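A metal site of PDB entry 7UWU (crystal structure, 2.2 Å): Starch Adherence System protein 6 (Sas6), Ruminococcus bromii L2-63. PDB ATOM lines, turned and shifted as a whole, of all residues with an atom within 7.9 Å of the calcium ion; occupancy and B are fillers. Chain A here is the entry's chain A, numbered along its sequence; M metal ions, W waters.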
ATOM      1  N   TYR A 212       4.939 -23.899 -11.048  1.00  0.00           N
ATOM      2  CA  TYR A 212       5.175 -22.522 -11.467  1.00  0.00           C
ATOM      3  C   TYR A 212       4.864 -22.360 -12.944  1.00  0.00           C
ATOM      4  O   TYR A 212       4.926 -23.316 -13.720  1.00  0.00           O
ATOM      5  CB  TYR A 212       6.643 -22.134 -11.246  1.00  0.00           C
ATOM      6  CG  TYR A 212       7.084 -22.230  -9.800  1.00  0.00           C
ATOM      7  CD1 TYR A 212       6.755 -21.233  -8.878  1.00  0.00           C
ATOM      8  CD2 TYR A 212       7.823 -23.320  -9.360  1.00  0.00           C
ATOM      9  CE1 TYR A 212       7.149 -21.316  -7.571  1.00  0.00           C
ATOM     10  CE2 TYR A 212       8.239 -23.409  -8.033  1.00  0.00           C
ATOM     11  CZ  TYR A 212       7.888 -22.404  -7.145  1.00  0.00           C
ATOM     12  OH  TYR A 212       8.310 -22.492  -5.840  1.00  0.00           O
ATOM     13  N   GLN A 243       2.130 -17.526 -12.387  1.00  0.00           N
ATOM     14  CA  GLN A 243       1.578 -18.481 -11.449  1.00  0.00           C
ATOM     15  C   GLN A 243       2.712 -18.949 -10.538  1.00  0.00           C
ATOM     16  O   GLN A 243       3.724 -19.461 -11.033  1.00  0.00           O
ATOM     17  CB  GLN A 243       0.947 -19.658 -12.201  1.00  0.00           C
ATOM     18  CG  GLN A 243       0.385 -20.768 -11.322  1.00  0.00           C
ATOM     19  CD  GLN A 243      -0.777 -20.305 -10.474  1.00  0.00           C
ATOM     20  OE1 GLN A 243      -1.814 -19.868 -10.977  1.00  0.00           O
ATOM     21  NE2 GLN A 243      -0.589 -20.391  -9.157  1.00  0.00           N
ATOM     22  N   GLY A 244       2.563 -18.721  -9.240  1.00  0.00           N
ATOM     23  CA  GLY A 244       3.449 -19.255  -8.247  1.00  0.00           C
ATOM     24  C   GLY A 244       2.827 -20.447  -7.548  1.00  0.00           C
ATOM     25  O   GLY A 244       1.856 -21.048  -8.025  1.00  0.00           O
ATOM     26  N   VAL A 245       3.380 -20.790  -6.389  1.00  0.00           N
ATOM     27  CA  VAL A 245       2.896 -21.894  -5.562  1.00  0.00           C
ATOM     28  C   VAL A 245       2.787 -21.414  -4.122  1.00  0.00           C
ATOM     29  O   VAL A 245       3.467 -20.472  -3.690  1.00  0.00           O
ATOM     30  CB  VAL A 245       3.841 -23.117  -5.627  1.00  0.00           C
ATOM     31  CG1 VAL A 245       4.349 -23.352  -7.040  1.00  0.00           C
ATOM     32  CG2 VAL A 245       5.014 -22.944  -4.677  1.00  0.00           C
ATOM     33  N   ALA A 246       1.951 -22.098  -3.344  1.00  0.00           N
ATOM     34  CA  ALA A 246       1.851 -21.810  -1.919  1.00  0.00           C
ATOM     35  C   ALA A 246       2.940 -22.522  -1.129  1.00  0.00           C
ATOM     36  O   ALA A 246       3.531 -23.521  -1.558  1.00  0.00           O
ATOM     37  CB  ALA A 246       0.479 -22.230  -1.363  1.00  0.00           C
ATOM     38  N   ASN A 247       3.155 -22.010   0.080  1.00  0.00           N
ATOM     39  CA  ASN A 247       3.990 -22.659   1.083  1.00  0.00           C
ATOM     40  C   ASN A 247       5.396 -22.891   0.584  1.00  0.00           C
ATOM     41  O   ASN A 247       6.037 -23.883   0.916  1.00  0.00           O
ATOM     42  CB  ASN A 247       3.377 -23.980   1.560  1.00  0.00           C
ATOM     43  CG  ASN A 247       3.835 -24.357   2.958  1.00  0.00           C
ATOM     44  OD1 ASN A 247       4.013 -23.494   3.811  1.00  0.00           O
ATOM     45  ND2 ASN A 247       4.019 -25.642   3.209  1.00  0.00           N
ATOM     46  N   ASP A 248       5.878 -21.959  -0.242  1.00  0.00           N
ATOM     47  CA  ASP A 248       7.264 -21.943  -0.668  1.00  0.00           C
ATOM     48  C   ASP A 248       7.969 -20.672  -0.206  1.00  0.00           C
ATOM     49  O   ASP A 248       8.991 -20.303  -0.775  1.00  0.00           O
ATOM     50  CB  ASP A 248       7.354 -22.075  -2.188  1.00  0.00           C
ATOM     51  CG  ASP A 248       6.793 -20.858  -2.902  1.00  0.00           C
ATOM     52  OD1 ASP A 248       6.106 -20.054  -2.244  1.00  0.00           O
ATOM     53  OD2 ASP A 248       6.994 -20.725  -4.130  1.00  0.00           O
ATOM     54  N   ASP A 249       7.422 -19.978   0.792  1.00  0.00           N
ATOM     55  CA  ASP A 249       8.102 -18.788   1.274  1.00  0.00           C
ATOM     56  C   ASP A 249       9.266 -19.198   2.184  1.00  0.00           C
ATOM     57  O   ASP A 249       9.316 -20.331   2.690  1.00  0.00           O
ATOM     58  CB  ASP A 249       7.138 -17.829   1.984  1.00  0.00           C
ATOM     59  CG  ASP A 249       6.211 -18.516   2.991  1.00  0.00           C
ATOM     60  OD1 ASP A 249       5.693 -19.621   2.715  1.00  0.00           O
ATOM     61  OD2 ASP A 249       5.995 -17.940   4.082  1.00  0.00           O
ATOM     62  N   PRO A 250      10.268 -18.331   2.343  1.00  0.00           N
ATOM     63  CA  PRO A 250      11.531 -18.774   2.976  1.00  0.00           C
ATOM     64  C   PRO A 250      11.366 -19.464   4.315  1.00  0.00           C
ATOM     65  O   PRO A 250      12.128 -20.398   4.609  1.00  0.00           O
ATOM     66  CB  PRO A 250      12.323 -17.459   3.121  1.00  0.00           C
ATOM     67  CG  PRO A 250      11.857 -16.631   1.968  1.00  0.00           C
ATOM     68  CD  PRO A 250      10.395 -16.980   1.752  1.00  0.00           C
ATOM     69  N   TRP A 263       4.766 -14.763   3.942  1.00  0.00           N
ATOM     70  CA  TRP A 263       4.805 -13.855   2.809  1.00  0.00           C
ATOM     71  C   TRP A 263       4.754 -14.719   1.540  1.00  0.00           C
ATOM     72  O   TRP A 263       5.755 -14.945   0.865  1.00  0.00           O
ATOM     73  CB  TRP A 263       6.043 -12.958   2.860  1.00  0.00           C
ATOM     74  CG  TRP A 263       5.888 -12.000   4.001  1.00  0.00           C
ATOM     75  CD1 TRP A 263       6.325 -12.178   5.281  1.00  0.00           C
ATOM     76  CD2 TRP A 263       5.201 -10.743   3.979  1.00  0.00           C
ATOM     77  NE1 TRP A 263       5.973 -11.100   6.057  1.00  0.00           N
ATOM     78  CE2 TRP A 263       5.272 -10.212   5.286  1.00  0.00           C
ATOM     79  CE3 TRP A 263       4.528 -10.016   2.989  1.00  0.00           C
ATOM     80  CZ2 TRP A 263       4.711  -8.971   5.615  1.00  0.00           C
ATOM     81  CZ3 TRP A 263       3.965  -8.787   3.331  1.00  0.00           C
ATOM     82  CH2 TRP A 263       4.062  -8.279   4.635  1.00  0.00           C
ATOM     83  N   ASP A 264       3.560 -15.217   1.236  1.00  0.00           N
ATOM     84  CA  ASP A 264       3.390 -16.314   0.284  1.00  0.00           C
ATOM     85  C   ASP A 264       2.580 -15.849  -0.912  1.00  0.00           C
ATOM     86  O   ASP A 264       1.343 -15.822  -0.868  1.00  0.00           O
ATOM     87  CB  ASP A 264       2.718 -17.498   0.978  1.00  0.00           C
ATOM     88  CG  ASP A 264       2.793 -18.766   0.150  1.00  0.00           C
ATOM     89  OD1 ASP A 264       3.460 -18.719  -0.898  1.00  0.00           O
ATOM     90  OD2 ASP A 264       2.162 -19.776   0.522  1.00  0.00           O
ATOM     91  N   ALA A 265       3.280 -15.499  -1.989  1.00  0.00           N
ATOM     92  CA  ALA A 265       2.615 -15.022  -3.200  1.00  0.00           C
ATOM     93  C   ALA A 265       2.047 -16.195  -3.975  1.00  0.00           C
ATOM     94  O   ALA A 265       2.770 -17.162  -4.225  1.00  0.00           O
ATOM     95  CB  ALA A 265       3.590 -14.226  -4.067  1.00  0.00           C
ATOM     96  N   TYR A 266       0.776 -16.146  -4.348  1.00  0.00           N
ATOM     97  CA  TYR A 266       0.251 -17.278  -5.083  1.00  0.00           C
ATOM     98  C   TYR A 266       0.072 -17.031  -6.574  1.00  0.00           C
ATOM     99  O   TYR A 266       0.386 -17.918  -7.376  1.00  0.00           O
ATOM    100  CB  TYR A 266      -1.066 -17.785  -4.459  1.00  0.00           C
ATOM    101  CG  TYR A 266      -1.413 -19.118  -5.079  1.00  0.00           C
ATOM    102  CD1 TYR A 266      -0.666 -20.263  -4.781  1.00  0.00           C
ATOM    103  CD2 TYR A 266      -2.435 -19.233  -6.011  1.00  0.00           C
ATOM    104  CE1 TYR A 266      -0.948 -21.486  -5.382  1.00  0.00           C
ATOM    105  CE2 TYR A 266      -2.733 -20.462  -6.627  1.00  0.00           C
ATOM    106  CZ  TYR A 266      -1.980 -21.581  -6.298  1.00  0.00           C
ATOM    107  OH  TYR A 266      -2.248 -22.809  -6.871  1.00  0.00           O
ATOM    108  N   ALA A 267      -0.391 -15.859  -7.003  1.00  0.00           N
ATOM    109  CA  ALA A 267      -0.648 -15.680  -8.429  1.00  0.00           C
ATOM    110  C   ALA A 267      -0.780 -14.202  -8.743  1.00  0.00           C
ATOM    111  O   ALA A 267      -1.234 -13.411  -7.907  1.00  0.00           O
ATOM    112  CB  ALA A 267      -1.904 -16.437  -8.883  1.00  0.00           C
ATOM    113  N   GLU A 282      -2.618 -12.567  -5.599  1.00  0.00           N
ATOM    114  CA  GLU A 282      -3.113 -13.535  -4.620  1.00  0.00           C
ATOM    115  C   GLU A 282      -1.972 -13.904  -3.691  1.00  0.00           C
ATOM    116  O   GLU A 282      -0.868 -14.219  -4.157  1.00  0.00           O
ATOM    117  CB  GLU A 282      -3.652 -14.781  -5.325  1.00  0.00           C
ATOM    118  CG  GLU A 282      -5.168 -14.804  -5.474  1.00  0.00           C
ATOM    119  CD  GLU A 282      -5.652 -15.985  -6.279  1.00  0.00           C
ATOM    120  OE1 GLU A 282      -5.042 -16.306  -7.334  1.00  0.00           O
ATOM    121  OE2 GLU A 282      -6.643 -16.616  -5.855  1.00  0.00           O
ATOM    122  N   MET A 283      -2.239 -13.863  -2.391  1.00  0.00           N
ATOM    123  CA  MET A 283      -1.324 -14.390  -1.397  1.00  0.00           C
ATOM    124  C   MET A 283      -2.027 -15.471  -0.598  1.00  0.00           C
ATOM    125  O   MET A 283      -3.192 -15.321  -0.214  1.00  0.00           O
ATOM    126  CB  MET A 283      -0.848 -13.305  -0.460  1.00  0.00           C
ATOM    127  CG  MET A 283       0.384 -12.621  -0.933  1.00  0.00           C
ATOM    128  SD  MET A 283       0.510 -10.918  -0.336  1.00  0.00           S
ATOM    129  CE  MET A 283       1.486 -11.235   1.137  1.00  0.00           C
ATOM    130  N   ALA A 284      -1.317 -16.566  -0.336  1.00  0.00           N
ATOM    131  CA  ALA A 284      -1.877 -17.681   0.406  1.00  0.00           C
ATOM    132  C   ALA A 284      -1.399 -17.661   1.858  1.00  0.00           C
ATOM    133  O   ALA A 284      -0.341 -17.115   2.185  1.00  0.00           O
ATOM    134  CB  ALA A 284      -1.511 -19.009  -0.243  1.00  0.00           C
ATOM    135  N   PHE A 428      -2.083 -25.003  -4.961  1.00  0.00           N
ATOM    136  CA  PHE A 428      -1.069 -26.050  -4.964  1.00  0.00           C
ATOM    137  C   PHE A 428       0.156 -25.612  -4.176  1.00  0.00           C
ATOM    138  O   PHE A 428       0.589 -24.456  -4.241  1.00  0.00           O
ATOM    139  CB  PHE A 428      -0.662 -26.390  -6.401  1.00  0.00           C
ATOM    140  CG  PHE A 428      -1.771 -26.909  -7.243  1.00  0.00           C
ATOM    141  CD1 PHE A 428      -2.295 -28.192  -7.027  1.00  0.00           C
ATOM    142  CD2 PHE A 428      -2.309 -26.129  -8.244  1.00  0.00           C
ATOM    143  CE1 PHE A 428      -3.325 -28.668  -7.810  1.00  0.00           C
ATOM    144  CE2 PHE A 428      -3.323 -26.598  -9.025  1.00  0.00           C
ATOM    145  CZ  PHE A 428      -3.838 -27.861  -8.814  1.00  0.00           C
ATOM    146  N   LEU A 492       7.663  -9.456  -3.065  1.00  0.00           N
ATOM    147  CA  LEU A 492       7.218  -9.328  -1.687  1.00  0.00           C
ATOM    148  C   LEU A 492       8.442  -9.289  -0.783  1.00  0.00           C
ATOM    149  O   LEU A 492       9.440  -9.969  -1.041  1.00  0.00           O
ATOM    150  CB  LEU A 492       6.306 -10.479  -1.262  1.00  0.00           C
ATOM    151  CG  LEU A 492       4.939 -10.625  -1.941  1.00  0.00           C
ATOM    152  CD1 LEU A 492       4.154 -11.783  -1.342  1.00  0.00           C
ATOM    153  CD2 LEU A 492       4.147  -9.336  -1.843  1.00  0.00           C
ATOM    154  N   MET A 499      11.277 -11.936  -0.500  1.00  0.00           N
ATOM    155  CA  MET A 499      10.906 -13.237   0.039  1.00  0.00           C
ATOM    156  C   MET A 499      10.267 -14.125  -1.000  1.00  0.00           C
ATOM    157  O   MET A 499      10.481 -15.334  -0.997  1.00  0.00           O
ATOM    158  CB  MET A 499       9.932 -13.103   1.222  1.00  0.00           C
ATOM    159  CG  MET A 499      10.420 -12.192   2.337  1.00  0.00           C
ATOM    160  SD  MET A 499      11.523 -13.044   3.445  1.00  0.00           S
ATOM    161  CE  MET A 499      10.372 -13.705   4.681  1.00  0.00           C
ATOM    162  N   ASP A 500       9.469 -13.554  -1.898  1.00  0.00           N
ATOM    163  CA  ASP A 500       8.708 -14.310  -2.876  1.00  0.00           C
ATOM    164  C   ASP A 500       8.496 -13.392  -4.066  1.00  0.00           C
ATOM    165  O   ASP A 500       8.368 -12.172  -3.905  1.00  0.00           O
ATOM    166  CB  ASP A 500       7.372 -14.792  -2.270  1.00  0.00           C
ATOM    167  CG  ASP A 500       6.728 -15.953  -3.049  1.00  0.00           C
ATOM    168  OD1 ASP A 500       7.108 -16.198  -4.211  1.00  0.00           O
ATOM    169  OD2 ASP A 500       5.811 -16.600  -2.486  1.00  0.00           O
ATOM    170  N   THR A 501       8.501 -13.965  -5.273  1.00  0.00           N
ATOM    171  CA  THR A 501       8.249 -13.180  -6.486  1.00  0.00           C
ATOM    172  C   THR A 501       7.310 -13.948  -7.411  1.00  0.00           C
ATOM    173  O   THR A 501       7.264 -15.184  -7.392  1.00  0.00           O
ATOM    174  CB  THR A 501       9.527 -12.864  -7.266  1.00  0.00           C
ATOM    175  OG1 THR A 501      10.175 -14.098  -7.582  1.00  0.00           O
ATOM    176  CG2 THR A 501      10.462 -11.992  -6.443  1.00  0.00           C
ATOM    177  N   LEU A 502       6.598 -13.185  -8.232  1.00  0.00           N
ATOM    178  CA  LEU A 502       5.806 -13.707  -9.352  1.00  0.00           C
ATOM    179  C   LEU A 502       6.179 -12.934 -10.607  1.00  0.00           C
ATOM    180  O   LEU A 502       5.931 -11.704 -10.657  1.00  0.00           O
ATOM    181  CB  LEU A 502       4.317 -13.550  -9.067  1.00  0.00           C
ATOM    182  CG  LEU A 502       3.764 -14.274  -7.844  1.00  0.00           C
ATOM    183  CD1 LEU A 502       2.347 -13.752  -7.553  1.00  0.00           C
ATOM    184  CD2 LEU A 502       3.764 -15.782  -8.079  1.00  0.00           C
ATOM    185  N   HIS A 504       8.178 -16.585 -10.119  1.00  0.00           N
ATOM    186  CA  HIS A 504       9.077 -16.939  -9.019  1.00  0.00           C
ATOM    187  C   HIS A 504      10.537 -16.899  -9.473  1.00  0.00           C
ATOM    188  O   HIS A 504      10.872 -17.390 -10.563  1.00  0.00           O
ATOM    189  CB  HIS A 504       8.736 -18.335  -8.478  1.00  0.00           C
ATOM    190  CG  HIS A 504       9.425 -18.661  -7.193  1.00  0.00           C
ATOM    191  ND1 HIS A 504      10.496 -19.522  -7.117  1.00  0.00           N
ATOM    192  CD2 HIS A 504       9.220 -18.209  -5.924  1.00  0.00           C
ATOM    193  CE1 HIS A 504      10.902 -19.611  -5.869  1.00  0.00           C
ATOM    194  NE2 HIS A 504      10.151 -18.829  -5.120  1.00  0.00           N
HETATM  195 CA    CA M   1       4.479 -18.448  -2.910  1.00  0.00          CA
HETATM  196  O   HOH W   1       5.768 -18.363  -5.228  1.00  0.00           O
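O of Asp 264 sits at hydrogen-bond distance from N of Ala 284 (2.8 Å). OD2 of Asp 248 sits at hydrogen-bond distance from OH of Tyr 212 (2.8 Å). The side-chain carboxylate (OD2) of Asp 264 sits at hydrogen-bond distance from the backbone NH (N) of Asn 247 (2.5 Å). The backbone carbonyl oxygen (O) of Asp 500 sits at hydrogen-bond distance from the backbone NH (N) of Leu 492.
The calcium ion is bound by OD1 of Asp 264 (2.3 Å), OD2 of Asp 500 (2.3 Å), OD1 of Asp 248 (2.4 Å), O of Val 245 (2.4 Å), O of Ala 265 (2.5 Å) and water W1 (2.7 Å).
Water W1 lies within hydrogen-bond range of OD1 of Asp 500 (2.7 Å) and OD2 of Asp 248 (2.9 Å).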
